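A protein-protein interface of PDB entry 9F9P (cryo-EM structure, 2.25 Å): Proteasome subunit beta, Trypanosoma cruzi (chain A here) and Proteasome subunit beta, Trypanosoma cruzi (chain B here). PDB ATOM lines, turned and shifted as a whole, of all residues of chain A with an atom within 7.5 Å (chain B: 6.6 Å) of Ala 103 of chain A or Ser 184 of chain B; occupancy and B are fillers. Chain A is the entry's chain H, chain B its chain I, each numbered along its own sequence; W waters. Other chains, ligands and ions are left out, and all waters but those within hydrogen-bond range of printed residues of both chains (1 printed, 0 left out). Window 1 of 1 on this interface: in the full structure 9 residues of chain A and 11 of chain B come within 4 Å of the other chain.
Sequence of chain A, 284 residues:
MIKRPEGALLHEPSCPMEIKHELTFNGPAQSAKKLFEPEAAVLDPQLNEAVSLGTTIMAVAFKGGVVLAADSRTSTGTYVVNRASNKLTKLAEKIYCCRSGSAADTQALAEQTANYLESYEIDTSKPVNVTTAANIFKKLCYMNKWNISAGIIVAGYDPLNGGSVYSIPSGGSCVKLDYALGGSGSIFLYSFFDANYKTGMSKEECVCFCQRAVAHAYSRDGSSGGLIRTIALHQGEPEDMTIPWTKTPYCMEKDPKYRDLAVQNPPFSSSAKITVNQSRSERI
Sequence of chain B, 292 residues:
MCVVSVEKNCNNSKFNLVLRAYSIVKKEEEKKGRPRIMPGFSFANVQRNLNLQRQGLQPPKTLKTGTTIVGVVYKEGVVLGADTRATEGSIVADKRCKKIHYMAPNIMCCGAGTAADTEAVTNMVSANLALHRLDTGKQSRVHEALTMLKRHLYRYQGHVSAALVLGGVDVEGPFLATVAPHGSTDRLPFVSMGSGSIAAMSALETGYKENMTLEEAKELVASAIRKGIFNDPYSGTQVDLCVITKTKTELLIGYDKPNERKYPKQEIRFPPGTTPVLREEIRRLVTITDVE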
ATOM      1  N   THR A  74     -15.213   8.095  21.915  1.00  0.00           N
ATOM      2  CA  THR A  74     -13.790   8.291  22.205  1.00  0.00           C
ATOM      3  C   THR A  74     -13.375   9.656  21.675  1.00  0.00           C
ATOM      4  O   THR A  74     -13.735  10.003  20.571  1.00  0.00           O
ATOM      5  CB  THR A  74     -12.939   7.162  21.590  1.00  0.00           C
ATOM      6  OG1 THR A  74     -13.277   5.882  22.141  1.00  0.00           O
ATOM      7  CG2 THR A  74     -11.454   7.349  21.833  1.00  0.00           C
ATOM      8  N   ARG A  99     -13.607  -0.531  30.244  1.00  0.00           N
ATOM      9  CA  ARG A  99     -12.329   0.144  30.153  1.00  0.00           C
ATOM     10  C   ARG A  99     -12.511   1.668  30.159  1.00  0.00           C
ATOM     11  O   ARG A  99     -13.329   2.183  29.404  1.00  0.00           O
ATOM     12  CB  ARG A  99     -11.644  -0.269  28.841  1.00  0.00           C
ATOM     13  CG  ARG A  99     -11.352  -1.752  28.649  1.00  0.00           C
ATOM     14  CD  ARG A  99     -10.549  -2.014  27.369  1.00  0.00           C
ATOM     15  NE  ARG A  99     -11.352  -1.925  26.157  1.00  0.00           N
ATOM     16  CZ  ARG A  99     -11.273  -0.936  25.288  1.00  0.00           C
ATOM     17  NH1 ARG A  99     -12.150  -0.840  24.302  1.00  0.00           N
ATOM     18  NH2 ARG A  99     -10.325  -0.018  25.433  1.00  0.00           N
ATOM     19  N   SER A 100     -11.729   2.377  30.994  1.00  0.00           N
ATOM     20  CA  SER A 100     -11.676   3.830  30.950  1.00  0.00           C
ATOM     21  C   SER A 100     -10.237   4.328  31.076  1.00  0.00           C
ATOM     22  O   SER A 100      -9.395   3.728  31.729  1.00  0.00           O
ATOM     23  CB  SER A 100     -12.553   4.486  32.031  1.00  0.00           C
ATOM     24  OG  SER A 100     -11.865   4.518  33.308  1.00  0.00           O
ATOM     25  N   GLY A 101     -10.008   5.519  30.532  1.00  0.00           N
ATOM     26  CA  GLY A 101      -8.687   6.109  30.494  1.00  0.00           C
ATOM     27  C   GLY A 101      -8.101   5.989  29.085  1.00  0.00           C
ATOM     28  O   GLY A 101      -8.842   6.036  28.105  1.00  0.00           O
ATOM     29  N   SER A 102      -6.781   5.814  29.010  1.00  0.00           N
ATOM     30  CA  SER A 102      -6.071   5.713  27.744  1.00  0.00           C
ATOM     31  C   SER A 102      -6.515   4.492  26.963  1.00  0.00           C
ATOM     32  O   SER A 102      -6.342   3.380  27.436  1.00  0.00           O
ATOM     33  CB  SER A 102      -4.594   5.639  27.980  1.00  0.00           C
ATOM     34  OG  SER A 102      -3.948   5.014  26.870  1.00  0.00           O
ATOM     35  N   ALA A 103      -7.019   4.691  25.752  1.00  0.00           N
ATOM     36  CA  ALA A 103      -7.394   3.561  24.906  1.00  0.00           C
ATOM     37  C   ALA A 103      -6.213   2.613  24.682  1.00  0.00           C
ATOM     38  O   ALA A 103      -6.394   1.399  24.697  1.00  0.00           O
ATOM     39  CB  ALA A 103      -7.920   4.060  23.586  1.00  0.00           C
ATOM     40  N   ALA A 104      -4.998   3.149  24.506  1.00  0.00           N
ATOM     41  CA  ALA A 104      -3.892   2.278  24.158  1.00  0.00           C
ATOM     42  C   ALA A 104      -3.570   1.355  25.326  1.00  0.00           C
ATOM     43  O   ALA A 104      -3.318   0.165  25.107  1.00  0.00           O
ATOM     44  CB  ALA A 104      -2.679   3.051  23.716  1.00  0.00           C
ATOM     45  N   ASP A 105      -3.592   1.903  26.554  1.00  0.00           N
ATOM     46  CA  ASP A 105      -3.174   1.157  27.743  1.00  0.00           C
ATOM     47  C   ASP A 105      -4.206   0.108  28.113  1.00  0.00           C
ATOM     48  O   ASP A 105      -3.853  -1.018  28.392  1.00  0.00           O
ATOM     49  CB  ASP A 105      -2.931   2.077  28.936  1.00  0.00           C
ATOM     50  CG  ASP A 105      -1.756   3.005  28.702  1.00  0.00           C
ATOM     51  OD1 ASP A 105      -0.690   2.468  28.309  1.00  0.00           O
ATOM     52  OD2 ASP A 105      -1.914   4.253  28.901  1.00  0.00           O
ATOM     53  N   THR A 106      -5.470   0.469  28.057  1.00  0.00           N
ATOM     54  CA  THR A 106      -6.485  -0.503  28.395  1.00  0.00           C
ATOM     55  C   THR A 106      -6.588  -1.614  27.351  1.00  0.00           C
ATOM     56  O   THR A 106      -6.918  -2.732  27.712  1.00  0.00           O
ATOM     57  CB  THR A 106      -7.841   0.168  28.659  1.00  0.00           C
ATOM     58  OG1 THR A 106      -8.381   0.805  27.491  1.00  0.00           O
ATOM     59  CG2 THR A 106      -7.706   1.127  29.824  1.00  0.00           C
ATOM     60  N   GLN A 107      -6.379  -1.322  26.067  1.00  0.00           N
ATOM     61  CA  GLN A 107      -6.448  -2.381  25.076  1.00  0.00           C
ATOM     62  C   GLN A 107      -5.294  -3.352  25.328  1.00  0.00           C
ATOM     63  O   GLN A 107      -5.496  -4.558  25.361  1.00  0.00           O
ATOM     64  CB  GLN A 107      -6.441  -1.869  23.644  1.00  0.00           C
ATOM     65  CG  GLN A 107      -7.728  -1.179  23.173  1.00  0.00           C
ATOM     66  CD  GLN A 107      -7.553  -0.652  21.744  1.00  0.00           C
ATOM     67  OE1 GLN A 107      -6.711  -1.144  20.987  1.00  0.00           O
ATOM     68  NE2 GLN A 107      -8.359   0.326  21.341  1.00  0.00           N
ATOM     69  N   ALA A 108      -4.101  -2.823  25.578  1.00  0.00           N
ATOM     70  CA  ALA A 108      -2.951  -3.672  25.778  1.00  0.00           C
ATOM     71  C   ALA A 108      -3.106  -4.532  27.024  1.00  0.00           C
ATOM     72  O   ALA A 108      -2.850  -5.706  26.933  1.00  0.00           O
ATOM     73  CB  ALA A 108      -1.697  -2.824  25.829  1.00  0.00           C
ATOM     74  N   LEU A 109      -3.532  -4.019  28.180  1.00  0.00           N
ATOM     75  CA  LEU A 109      -3.669  -4.857  29.378  1.00  0.00           C
ATOM     76  C   LEU A 109      -4.848  -5.830  29.312  1.00  0.00           C
ATOM     77  O   LEU A 109      -4.803  -6.880  29.942  1.00  0.00           O
ATOM     78  CB  LEU A 109      -3.787  -3.990  30.646  1.00  0.00           C
ATOM     79  CG  LEU A 109      -2.586  -3.075  30.978  1.00  0.00           C
ATOM     80  CD1 LEU A 109      -2.634  -2.578  32.406  1.00  0.00           C
ATOM     81  CD2 LEU A 109      -1.224  -3.744  30.756  1.00  0.00           C
ATOM     82  N   SER A 149      -2.717   5.237  32.321  1.00  0.00           N
ATOM     83  CA  SER A 149      -3.956   5.856  32.741  1.00  0.00           C
ATOM     84  C   SER A 149      -5.117   4.873  32.529  1.00  0.00           C
ATOM     85  O   SER A 149      -5.618   4.726  31.415  1.00  0.00           O
ATOM     86  CB  SER A 149      -4.180   7.171  32.010  1.00  0.00           C
ATOM     87  OG  SER A 149      -5.570   7.525  31.984  1.00  0.00           O
ATOM     88  N   LYS B 150       0.152  -2.605  15.769  1.00  0.00           N
ATOM     89  CA  LYS B 150      -0.225  -2.177  17.106  1.00  0.00           C
ATOM     90  C   LYS B 150       0.813  -2.556  18.160  1.00  0.00           C
ATOM     91  O   LYS B 150       1.056  -1.770  19.046  1.00  0.00           O
ATOM     92  CB  LYS B 150      -1.671  -2.654  17.338  1.00  0.00           C
ATOM     93  CG  LYS B 150      -2.033  -3.140  18.712  1.00  0.00           C
ATOM     94  CD  LYS B 150      -3.209  -4.099  18.686  1.00  0.00           C
ATOM     95  CE  LYS B 150      -4.546  -3.397  18.777  1.00  0.00           C
ATOM     96  NZ  LYS B 150      -4.715  -2.720  20.091  1.00  0.00           N
ATOM     97  N   LEU B 153       3.989  -0.257  17.759  1.00  0.00           N
ATOM     98  CA  LEU B 153       3.745   1.119  18.149  1.00  0.00           C
ATOM     99  C   LEU B 153       3.612   1.255  19.662  1.00  0.00           C
ATOM    100  O   LEU B 153       4.189   2.195  20.209  1.00  0.00           O
ATOM    101  CB  LEU B 153       2.517   1.657  17.432  1.00  0.00           C
ATOM    102  CG  LEU B 153       2.740   1.878  15.940  1.00  0.00           C
ATOM    103  CD1 LEU B 153       1.481   2.356  15.271  1.00  0.00           C
ATOM    104  CD2 LEU B 153       3.843   2.882  15.701  1.00  0.00           C
ATOM    105  N   TYR B 154       2.948   0.290  20.319  1.00  0.00           N
ATOM    106  CA  TYR B 154       2.746   0.321  21.761  1.00  0.00           C
ATOM    107  C   TYR B 154       4.081   0.260  22.505  1.00  0.00           C
ATOM    108  O   TYR B 154       4.234   0.986  23.480  1.00  0.00           O
ATOM    109  CB  TYR B 154       1.795  -0.795  22.255  1.00  0.00           C
ATOM    110  CG  TYR B 154       1.452  -0.692  23.721  1.00  0.00           C
ATOM    111  CD1 TYR B 154       0.733   0.400  24.167  1.00  0.00           C
ATOM    112  CD2 TYR B 154       1.977  -1.530  24.681  1.00  0.00           C
ATOM    113  CE1 TYR B 154       0.473   0.629  25.508  1.00  0.00           C
ATOM    114  CE2 TYR B 154       1.717  -1.340  26.036  1.00  0.00           C
ATOM    115  CZ  TYR B 154       0.952  -0.255  26.452  1.00  0.00           C
ATOM    116  OH  TYR B 154       0.582   0.076  27.746  1.00  0.00           O
ATOM    117  N   THR B 178      -8.076   1.999  11.746  1.00  0.00           N
ATOM    118  CA  THR B 178      -7.032   2.968  12.024  1.00  0.00           C
ATOM    119  C   THR B 178      -6.109   2.502  13.130  1.00  0.00           C
ATOM    120  O   THR B 178      -6.513   1.764  13.995  1.00  0.00           O
ATOM    121  CB  THR B 178      -7.584   4.306  12.519  1.00  0.00           C
ATOM    122  OG1 THR B 178      -8.462   4.141  13.641  1.00  0.00           O
ATOM    123  CG2 THR B 178      -8.375   5.025  11.455  1.00  0.00           C
ATOM    124  N   VAL B 179      -4.886   3.011  13.139  1.00  0.00           N
ATOM    125  CA  VAL B 179      -3.965   2.767  14.241  1.00  0.00           C
ATOM    126  C   VAL B 179      -3.353   4.110  14.604  1.00  0.00           C
ATOM    127  O   VAL B 179      -2.792   4.764  13.756  1.00  0.00           O
ATOM    128  CB  VAL B 179      -2.859   1.778  13.834  1.00  0.00           C
ATOM    129  CG1 VAL B 179      -2.051   1.271  15.027  1.00  0.00           C
ATOM    130  CG2 VAL B 179      -3.447   0.616  13.035  1.00  0.00           C
ATOM    131  N   ALA B 180      -3.543   4.526  15.850  1.00  0.00           N
ATOM    132  CA  ALA B 180      -3.001   5.768  16.387  1.00  0.00           C
ATOM    133  C   ALA B 180      -1.561   5.521  16.799  1.00  0.00           C
ATOM    134  O   ALA B 180      -1.170   4.385  16.960  1.00  0.00           O
ATOM    135  CB  ALA B 180      -3.839   6.218  17.570  1.00  0.00           C
ATOM    136  N   PRO B 181      -0.724   6.558  16.979  1.00  0.00           N
ATOM    137  CA  PRO B 181       0.680   6.374  17.355  1.00  0.00           C
ATOM    138  C   PRO B 181       0.969   5.703  18.701  1.00  0.00           C
ATOM    139  O   PRO B 181       2.057   5.149  18.867  1.00  0.00           O
ATOM    140  CB  PRO B 181       1.231   7.795  17.443  1.00  0.00           C
ATOM    141  CG  PRO B 181       0.281   8.613  16.644  1.00  0.00           C
ATOM    142  CD  PRO B 181      -1.079   7.970  16.824  1.00  0.00           C
ATOM    143  N   HIS B 182       0.048   5.801  19.675  1.00  0.00           N
ATOM    144  CA  HIS B 182       0.290   5.195  20.979  1.00  0.00           C
ATOM    145  C   HIS B 182      -0.056   3.715  20.929  1.00  0.00           C
ATOM    146  O   HIS B 182       0.202   3.011  21.879  1.00  0.00           O
ATOM    147  CB  HIS B 182      -0.462   5.951  22.085  1.00  0.00           C
ATOM    148  CG  HIS B 182       0.218   7.232  22.498  1.00  0.00           C
ATOM    149  ND1 HIS B 182      -0.101   8.452  21.939  1.00  0.00           N
ATOM    150  CD2 HIS B 182       1.256   7.463  23.350  1.00  0.00           C
ATOM    151  CE1 HIS B 182       0.716   9.379  22.431  1.00  0.00           C
ATOM    152  NE2 HIS B 182       1.552   8.799  23.286  1.00  0.00           N
ATOM    153  N   GLY B 183      -0.705   3.265  19.846  1.00  0.00           N
ATOM    154  CA  GLY B 183      -0.935   1.853  19.624  1.00  0.00           C
ATOM    155  C   GLY B 183      -2.378   1.418  19.806  1.00  0.00           C
ATOM    156  O   GLY B 183      -2.625   0.230  19.931  1.00  0.00           O
ATOM    157  N   SER B 184      -3.330   2.346  19.796  1.00  0.00           N
ATOM    158  CA  SER B 184      -4.730   1.973  19.906  1.00  0.00           C
ATOM    159  C   SER B 184      -5.334   1.789  18.522  1.00  0.00           C
ATOM    160  O   SER B 184      -4.947   2.478  17.598  1.00  0.00           O
ATOM    161  CB  SER B 184      -5.529   2.977  20.753  1.00  0.00           C
ATOM    162  OG  SER B 184      -5.476   4.296  20.233  1.00  0.00           O
ATOM    163  N   THR B 185      -6.335   0.918  18.409  1.00  0.00           N
ATOM    164  CA  THR B 185      -7.010   0.666  17.145  1.00  0.00           C
ATOM    165  C   THR B 185      -8.524   0.820  17.195  1.00  0.00           C
ATOM    166  O   THR B 185      -9.117   0.795  18.263  1.00  0.00           O
ATOM    167  CB  THR B 185      -6.757  -0.774  16.691  1.00  0.00           C
ATOM    168  OG1 THR B 185      -7.303  -1.678  17.656  1.00  0.00           O
ATOM    169  CG2 THR B 185      -5.271  -1.010  16.512  1.00  0.00           C
ATOM    170  N   ASP B 186      -9.118   0.918  16.002  1.00  0.00           N
ATOM    171  CA  ASP B 186     -10.546   1.100  15.806  1.00  0.00           C
ATOM    172  C   ASP B 186     -10.896   0.498  14.460  1.00  0.00           C
ATOM    173  O   ASP B 186     -10.283   0.851  13.466  1.00  0.00           O
ATOM    174  CB  ASP B 186     -10.945   2.575  15.737  1.00  0.00           C
ATOM    175  CG  ASP B 186     -10.741   3.401  17.016  1.00  0.00           C
ATOM    176  OD1 ASP B 186     -11.426   3.097  18.061  1.00  0.00           O
ATOM    177  OD2 ASP B 186      -9.942   4.379  16.971  1.00  0.00           O
HETATM  178  O   HOH W   1      -2.732  -1.104  22.505  1.00  0.00           O
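The side-chain amide nitrogen of Gln 107 of chain A sits at hydrogen-bond distance from the backbone carbonyl oxygen of Thr 185 of chain B, 3.2 Å away. OD1 of Asp 105 of chain A sits at hydrogen-bond distance from OH of Tyr 154 of chain B. OE1 of Gln 107 of chain A is in hydrogen-bond range of NZ of Lys 150 of chain B (2.7 Å).
The side-chain hydroxyl of Ser 102 of chain A is in hydrogen-bond range of the side-chain carboxylate of Asp 105 of chain A. The backbone carbonyl oxygen (O) of Ala 103 of chain A is in hydrogen-bond range of the side-chain hydroxyl (OG1) of Thr 106 of chain A, at 3.5 Å. N of Ala 104 of chain A lies close to OG of Ser 102 of chain A, at 3.2 Å.
Ala 103 of chain A touches Ser 184 of chain B. Ala 104 of chain A touches Tyr 154 of chain B (O to CE1, 3.8 Å). Ala 104 of chain A touches His 182 of chain B. Ser 184 of chain B touches Ala 104 of chain A (CB to N, 3.8 Å). Ser 184 of chain B touches Gln 107 of chain A. Ala 108 of chain A touches Tyr 154 of chain B.
Printed residues of chain B within 4 Å of Asp 105 of chain A: Tyr 154. Printed residues of chain B within 4 Å of Gln 107 of chain A: Lys 150 (2.7 Å), Ser 184 (3.8 Å) and Thr 185 (3.2 Å). Leu 153 of chain B touches none of the printed residues of chain A. Of the printed residues of chain A, Tyr 154 of chain B touches Ala 104 (3.8 Å), Asp 105 (2.8 Å) and Ala 108 (3.7 Å). Ala 180 of chain B touches none of the printed residues of chain A. Gly 183 of chain B touches none of the printed residues of chain A. Ser 184 of chain B touches just these residues of chain A: Ala 103 (3.9 Å), Ala 104 (3.8 Å) and Gln 107 (3.8 Å). Printed residues of chain A within 4 Å of Thr 185 of chain B: Gln 107 (3.2 Å). The nearest residue of chain A that does not touch Ser 184 of chain B is Asp 105 of chain A (6.2 Å). The nearest printed residue of chain B that does not touch Asp 105 of chain A is His 182 of chain B (6.1 Å).
Hydrophobic or aromatic side chains of chain B that line the printed part of chain A: Tyr 154 and His 182. Printed residues of chain A that touch a printed residue of chain B: Ala 103, Ala 104, Asp 105, Gln 107 and Ala 108. Hydrophobic or aromatic side chains of chain A within 4 Å of the printed part of chain B: Ala 103, Ala 104 and Ala 108. Among the printed residues, no Asp or Glu carboxylate lies within 4 Å of a Lys or Arg side-chain nitrogen of the other chain.
Water W1 bridges the backbone carbonyl oxygen of Gly 183 of chain B (2.9 Å) and the backbone carbonyl oxygen of Ala 104 of chain A (3.0 Å).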
